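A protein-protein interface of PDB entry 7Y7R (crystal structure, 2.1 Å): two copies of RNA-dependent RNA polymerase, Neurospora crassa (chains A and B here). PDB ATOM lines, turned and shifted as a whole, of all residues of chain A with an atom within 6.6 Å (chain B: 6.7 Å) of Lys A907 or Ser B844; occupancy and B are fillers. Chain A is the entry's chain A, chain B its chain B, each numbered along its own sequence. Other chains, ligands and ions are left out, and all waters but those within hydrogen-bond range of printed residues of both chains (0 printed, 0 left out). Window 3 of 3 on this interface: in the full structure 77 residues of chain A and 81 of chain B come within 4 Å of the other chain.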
ATOM      1  N   SER A 906      13.110 -32.632   1.949  1.00  0.00           N
ATOM      2  CA  SER A 906      14.427 -32.342   2.513  1.00  0.00           C
ATOM      3  C   SER A 906      14.420 -32.387   4.041  1.00  0.00           C
ATOM      4  O   SER A 906      15.353 -32.907   4.653  1.00  0.00           O
ATOM      5  CB  SER A 906      14.933 -30.982   2.044  1.00  0.00           C
ATOM      6  OG  SER A 906      16.307 -30.847   2.356  1.00  0.00           O
ATOM      7  N   LYS A 907      13.374 -31.824   4.657  1.00  0.00           N
ATOM      8  CA  LYS A 907      13.159 -32.050   6.083  1.00  0.00           C
ATOM      9  C   LYS A 907      12.715 -33.482   6.354  1.00  0.00           C
ATOM     10  O   LYS A 907      13.084 -34.067   7.381  1.00  0.00           O
ATOM     11  CB  LYS A 907      12.126 -31.068   6.626  1.00  0.00           C
ATOM     12  CG  LYS A 907      12.502 -29.633   6.410  1.00  0.00           C
ATOM     13  CD  LYS A 907      11.587 -28.709   7.193  1.00  0.00           C
ATOM     14  CE  LYS A 907      10.377 -28.315   6.373  1.00  0.00           C
ATOM     15  NZ  LYS A 907      10.710 -28.124   4.931  1.00  0.00           N
ATOM     16  N   VAL A 908      11.935 -34.058   5.437  1.00  0.00           N
ATOM     17  CA  VAL A 908      11.526 -35.453   5.568  1.00  0.00           C
ATOM     18  C   VAL A 908      12.742 -36.374   5.541  1.00  0.00           C
ATOM     19  O   VAL A 908      12.815 -37.348   6.302  1.00  0.00           O
ATOM     20  CB  VAL A 908      10.512 -35.810   4.464  1.00  0.00           C
ATOM     21  CG1 VAL A 908      10.346 -37.328   4.344  1.00  0.00           C
ATOM     22  CG2 VAL A 908       9.176 -35.124   4.732  1.00  0.00           C
ATOM     23  N   ILE A 909      13.720 -36.083   4.674  1.00  0.00           N
ATOM     24  CA  ILE A 909      14.918 -36.921   4.621  1.00  0.00           C
ATOM     25  C   ILE A 909      15.746 -36.744   5.886  1.00  0.00           C
ATOM     26  O   ILE A 909      16.231 -37.722   6.472  1.00  0.00           O
ATOM     27  CB  ILE A 909      15.751 -36.618   3.363  1.00  0.00           C
ATOM     28  CG1 ILE A 909      14.944 -36.908   2.095  1.00  0.00           C
ATOM     29  CG2 ILE A 909      17.035 -37.439   3.386  1.00  0.00           C
ATOM     30  CD1 ILE A 909      14.115 -35.709   1.594  1.00  0.00           C
ATOM     31  N   ARG A 910      15.921 -35.497   6.329  1.00  0.00           N
ATOM     32  CA  ARG A 910      16.637 -35.265   7.580  1.00  0.00           C
ATOM     33  C   ARG A 910      15.934 -35.952   8.742  1.00  0.00           C
ATOM     34  O   ARG A 910      16.587 -36.565   9.599  1.00  0.00           O
ATOM     35  CB  ARG A 910      16.782 -33.763   7.835  1.00  0.00           C
ATOM     36  CG  ARG A 910      18.142 -33.202   7.404  1.00  0.00           C
ATOM     37  CD  ARG A 910      18.035 -31.785   6.844  1.00  0.00           C
ATOM     38  NE  ARG A 910      18.244 -30.763   7.865  1.00  0.00           N
ATOM     39  CZ  ARG A 910      19.372 -30.088   8.039  1.00  0.00           C
ATOM     40  NH1 ARG A 910      20.429 -30.294   7.268  1.00  0.00           N
ATOM     41  NH2 ARG A 910      19.442 -29.179   9.010  1.00  0.00           N
ATOM     42  N   LEU A 911      14.597 -35.888   8.771  1.00  0.00           N
ATOM     43  CA  LEU A 911      13.855 -36.500   9.869  1.00  0.00           C
ATOM     44  C   LEU A 911      13.901 -38.021   9.818  1.00  0.00           C
ATOM     45  O   LEU A 911      13.864 -38.674  10.866  1.00  0.00           O
ATOM     46  CB  LEU A 911      12.414 -36.014   9.860  1.00  0.00           C
ATOM     47  CG  LEU A 911      12.243 -34.754  10.702  1.00  0.00           C
ATOM     48  CD1 LEU A 911      11.082 -33.926  10.185  1.00  0.00           C
ATOM     49  CD2 LEU A 911      12.047 -35.142  12.147  1.00  0.00           C
ATOM     50  N   LEU A 912      13.968 -38.603   8.619  1.00  0.00           N
ATOM     51  CA  LEU A 912      14.143 -40.044   8.514  1.00  0.00           C
ATOM     52  C   LEU A 912      15.569 -40.459   8.854  1.00  0.00           C
ATOM     53  O   LEU A 912      15.774 -41.528   9.443  1.00  0.00           O
ATOM     54  CB  LEU A 912      13.779 -40.522   7.101  1.00  0.00           C
ATOM     55  CG  LEU A 912      12.333 -40.320   6.617  1.00  0.00           C
ATOM     56  CD1 LEU A 912      12.096 -40.968   5.261  1.00  0.00           C
ATOM     57  CD2 LEU A 912      11.332 -40.857   7.632  1.00  0.00           C
ATOM     58  N   PHE B 833      19.648 -31.061  16.533  1.00  0.00           N
ATOM     59  CA  PHE B 833      19.097 -31.482  15.244  1.00  0.00           C
ATOM     60  C   PHE B 833      17.984 -30.550  14.789  1.00  0.00           C
ATOM     61  O   PHE B 833      18.024 -30.006  13.679  1.00  0.00           O
ATOM     62  CB  PHE B 833      18.574 -32.915  15.340  1.00  0.00           C
ATOM     63  CG  PHE B 833      17.689 -33.330  14.185  1.00  0.00           C
ATOM     64  CD1 PHE B 833      18.247 -33.785  12.989  1.00  0.00           C
ATOM     65  CD2 PHE B 833      16.307 -33.302  14.305  1.00  0.00           C
ATOM     66  CE1 PHE B 833      17.444 -34.191  11.930  1.00  0.00           C
ATOM     67  CE2 PHE B 833      15.492 -33.705  13.243  1.00  0.00           C
ATOM     68  CZ  PHE B 833      16.064 -34.150  12.056  1.00  0.00           C
ATOM     69  N   PHE B 834      16.977 -30.352  15.642  1.00  0.00           N
ATOM     70  CA  PHE B 834      15.838 -29.534  15.244  1.00  0.00           C
ATOM     71  C   PHE B 834      16.195 -28.054  15.197  1.00  0.00           C
ATOM     72  O   PHE B 834      15.557 -27.289  14.462  1.00  0.00           O
ATOM     73  CB  PHE B 834      14.651 -29.768  16.180  1.00  0.00           C
ATOM     74  CG  PHE B 834      13.331 -29.543  15.518  1.00  0.00           C
ATOM     75  CD1 PHE B 834      12.846 -30.457  14.590  1.00  0.00           C
ATOM     76  CD2 PHE B 834      12.590 -28.404  15.789  1.00  0.00           C
ATOM     77  CE1 PHE B 834      11.640 -30.248  13.957  1.00  0.00           C
ATOM     78  CE2 PHE B 834      11.377 -28.190  15.162  1.00  0.00           C
ATOM     79  CZ  PHE B 834      10.903 -29.112  14.240  1.00  0.00           C
ATOM     80  N   ILE B 837      17.364 -27.408  11.592  1.00  0.00           N
ATOM     81  CA  ILE B 837      16.184 -27.354  10.681  1.00  0.00           C
ATOM     82  C   ILE B 837      15.442 -26.037  10.917  1.00  0.00           C
ATOM     83  O   ILE B 837      15.052 -25.408   9.926  1.00  0.00           O
ATOM     84  CB  ILE B 837      15.279 -28.585  10.893  1.00  0.00           C
ATOM     85  CG1 ILE B 837      16.030 -29.894  10.640  1.00  0.00           C
ATOM     86  CG2 ILE B 837      14.014 -28.494  10.058  1.00  0.00           C
ATOM     87  CD1 ILE B 837      15.126 -31.077  10.404  1.00  0.00           C
ATOM     88  N   SER B 838      15.299 -25.622  12.178  1.00  0.00           N
ATOM     89  CA  SER B 838      14.546 -24.387  12.521  1.00  0.00           C
ATOM     90  C   SER B 838      15.229 -23.152  11.928  1.00  0.00           C
ATOM     91  O   SER B 838      14.516 -22.235  11.512  1.00  0.00           O
ATOM     92  CB  SER B 838      14.350 -24.263  14.001  1.00  0.00           C
ATOM     93  OG  SER B 838      15.210 -23.279  14.548  1.00  0.00           O
ATOM     94  N   LYS B 840      16.803 -22.763   9.157  1.00  0.00           N
ATOM     95  CA  LYS B 840      16.504 -22.631   7.707  1.00  0.00           C
ATOM     96  C   LYS B 840      14.996 -22.626   7.409  1.00  0.00           C
ATOM     97  O   LYS B 840      14.656 -22.384   6.242  1.00  0.00           O
ATOM     98  N   SER B 841      14.123 -22.895   8.386  1.00  0.00           N
ATOM     99  CA  SER B 841      12.664 -22.813   8.105  1.00  0.00           C
ATOM    100  C   SER B 841      11.904 -22.034   9.180  1.00  0.00           C
ATOM    101  O   SER B 841      11.998 -22.417  10.349  1.00  0.00           O
ATOM    102  CB  SER B 841      12.062 -24.175   7.897  1.00  0.00           C
ATOM    103  OG  SER B 841      12.571 -25.102   8.840  1.00  0.00           O
ATOM    104  N   ARG B 842      11.152 -21.004   8.782  1.00  0.00           N
ATOM    105  CA  ARG B 842      10.311 -20.234   9.736  1.00  0.00           C
ATOM    106  C   ARG B 842       9.190 -21.122  10.282  1.00  0.00           C
ATOM    107  O   ARG B 842       8.909 -21.030  11.487  1.00  0.00           O
ATOM    108  N   SER B 843       8.580 -21.940   9.425  1.00  0.00           N
ATOM    109  CA  SER B 843       7.440 -22.799   9.849  1.00  0.00           C
ATOM    110  C   SER B 843       7.887 -23.708  10.993  1.00  0.00           C
ATOM    111  O   SER B 843       7.186 -23.756  12.014  1.00  0.00           O
ATOM    112  N   SER B 844       9.027 -24.374  10.830  1.00  0.00           N
ATOM    113  CA  SER B 844       9.541 -25.284  11.886  1.00  0.00           C
ATOM    114  C   SER B 844      10.015 -24.483  13.109  1.00  0.00           C
ATOM    115  O   SER B 844       9.853 -24.979  14.229  1.00  0.00           O
ATOM    116  CB  SER B 844      10.599 -26.193  11.326  1.00  0.00           C
ATOM    117  OG  SER B 844      10.291 -26.561   9.992  1.00  0.00           O
ATOM    118  N   ALA B 845      10.551 -23.281  12.900  1.00  0.00           N
ATOM    119  CA  ALA B 845      11.037 -22.428  14.011  1.00  0.00           C
ATOM    120  C   ALA B 845       9.890 -22.020  14.935  1.00  0.00           C
ATOM    121  O   ALA B 845      10.107 -21.940  16.147  1.00  0.00           O
ATOM    122  CB  ALA B 845      11.753 -21.222  13.476  1.00  0.00           C
ATOM    123  N   LEU B 846       8.730 -21.724  14.359  1.00  0.00           N
ATOM    124  CA  LEU B 846       7.569 -21.332  15.191  1.00  0.00           C
ATOM    125  C   LEU B 846       7.205 -22.504  16.103  1.00  0.00           C
ATOM    126  O   LEU B 846       6.996 -22.270  17.300  1.00  0.00           O
ATOM    127  CB  LEU B 846       6.401 -20.948  14.280  1.00  0.00           C
ATOM    128  CG  LEU B 846       5.128 -20.509  15.000  1.00  0.00           C
ATOM    129  CD1 LEU B 846       5.379 -19.264  15.838  1.00  0.00           C
ATOM    130  CD2 LEU B 846       4.001 -20.267  14.009  1.00  0.00           C
ATOM    131  N   LEU B 847       7.189 -23.720  15.558  1.00  0.00           N
ATOM    132  CA  LEU B 847       6.832 -24.914  16.363  1.00  0.00           C
ATOM    133  C   LEU B 847       7.874 -25.066  17.465  1.00  0.00           C
ATOM    134  O   LEU B 847       7.488 -25.353  18.601  1.00  0.00           O
ATOM    135  CB  LEU B 847       6.824 -26.130  15.437  1.00  0.00           C
ATOM    136  CG  LEU B 847       6.502 -27.471  16.088  1.00  0.00           C
ATOM    137  CD1 LEU B 847       5.007 -27.740  16.042  1.00  0.00           C
ATOM    138  CD2 LEU B 847       7.263 -28.589  15.397  1.00  0.00           C
ATOM    139  N   PHE B 848       9.139 -24.850  17.122  1.00  0.00           N
ATOM    140  CA  PHE B 848      10.240 -25.009  18.099  1.00  0.00           C
ATOM    141  C   PHE B 848      10.104 -23.982  19.222  1.00  0.00           C
ATOM    142  O   PHE B 848      10.311 -24.345  20.387  1.00  0.00           O
ATOM    143  CB  PHE B 848      11.581 -24.907  17.373  1.00  0.00           C
ATOM    144  CG  PHE B 848      12.735 -25.599  18.048  1.00  0.00           C
ATOM    145  CD1 PHE B 848      12.527 -26.685  18.880  1.00  0.00           C
ATOM    146  CD2 PHE B 848      14.034 -25.168  17.837  1.00  0.00           C
ATOM    147  CE1 PHE B 848      13.594 -27.318  19.494  1.00  0.00           C
ATOM    148  CE2 PHE B 848      15.099 -25.804  18.451  1.00  0.00           C
ATOM    149  CZ  PHE B 848      14.876 -26.879  19.273  1.00  0.00           C
ATOM    150  N   THR B 849       9.758 -22.745  18.873  1.00  0.00           N
ATOM    151  CA  THR B 849       9.660 -21.668  19.886  1.00  0.00           C
ATOM    152  C   THR B 849       8.464 -21.976  20.775  1.00  0.00           C
ATOM    153  O   THR B 849       8.581 -21.829  21.990  1.00  0.00           O
ATOM    154  CB  THR B 849       9.619 -20.292  19.216  1.00  0.00           C
ATOM    155  OG1 THR B 849       8.653 -20.317  18.168  1.00  0.00           O
ATOM    156  CG2 THR B 849      10.963 -19.873  18.664  1.00  0.00           C
ATOM    157  N   VAL B 908       6.253 -32.776   8.565  1.00  0.00           N
ATOM    158  CA  VAL B 908       7.077 -32.681   9.801  1.00  0.00           C
ATOM    159  C   VAL B 908       6.240 -33.106  11.009  1.00  0.00           C
ATOM    160  O   VAL B 908       6.731 -33.923  11.784  1.00  0.00           O
ATOM    161  CB  VAL B 908       7.666 -31.267   9.967  1.00  0.00           C
ATOM    162  CG1 VAL B 908       8.117 -30.986  11.390  1.00  0.00           C
ATOM    163  CG2 VAL B 908       8.802 -31.016   8.991  1.00  0.00           C
ATOM    164  N   LEU B 911       5.546 -36.935  10.957  1.00  0.00           N
ATOM    165  CA  LEU B 911       6.786 -37.683  11.265  1.00  0.00           C
ATOM    166  C   LEU B 911       7.147 -37.491  12.742  1.00  0.00           C
ATOM    167  O   LEU B 911       7.639 -38.444  13.350  1.00  0.00           O
ATOM    168  CB  LEU B 911       7.898 -37.200  10.334  1.00  0.00           C
ATOM    169  CG  LEU B 911       8.036 -37.964   9.022  1.00  0.00           C
ATOM    170  CD1 LEU B 911       9.105 -37.334   8.149  1.00  0.00           C
ATOM    171  CD2 LEU B 911       8.365 -39.422   9.287  1.00  0.00           C
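Leu A911 touches Val B908, but with the chains exchanged Val A908 does not touch Leu B911 (4.002 Å). Leu A911 touches its own counterpart, Leu B911. 2 positions are printed for both chains. Of the 8 pairs that touch across the chains among the printed residues, 1 has its exchanged pair printed and touching as well.
Lys A907 touches Ile B837 (CD to CG2, 3.8 Å). Lys A907 touches Ser B844 (CD to OG, 3.8 Å). O of Arg A910 touches CE1 of Phe B833 (3.4 Å). NE of Arg A910 touches CG1 of Ile B837, 3.7 Å away. Phe B833 touches Leu A911. CD1 of Leu A911 touches CG2 of Val B908, 3.9 Å away. CB of Leu A911 touches CD1 of Leu B911, at 3.95 Å. Leu A912 touches Leu B911.
Of the 16 printed residues of chain B, 5 touch a printed residue of chain A. Printed residues of chain A that touch a printed residue of chain B: Lys A907, Arg A910, Leu A911 and Leu A912.
O of Ile B837 lies within hydrogen-bond range of OG of Ser B841 (2.7 Å). The side-chain hydroxyl (OG) of Ser B841 sits at hydrogen-bond distance from the side-chain hydroxyl (OG) of Ser B844, 2.9 Å away.
Of the printed residues of chain B, Lys A907 touches Ile B837 (3.8 Å) and Ser B844 (3.8 Å). Of chain A, only Lys A907 comes within 4 Å of Ser B844. Of the printed residues of chain A, Phe B833 touches Arg A910 (3.4 Å) and Leu A911 (3.9 Å). Printed residues of chain B within 4 Å of Leu A911: Phe B833, Val B908 and Leu B911. Printed residues of chain B within 4 Å of Leu A912: Leu B911. The nearest printed residue of chain A that does not touch Ser B844 is Leu A911 (7.4 Å).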
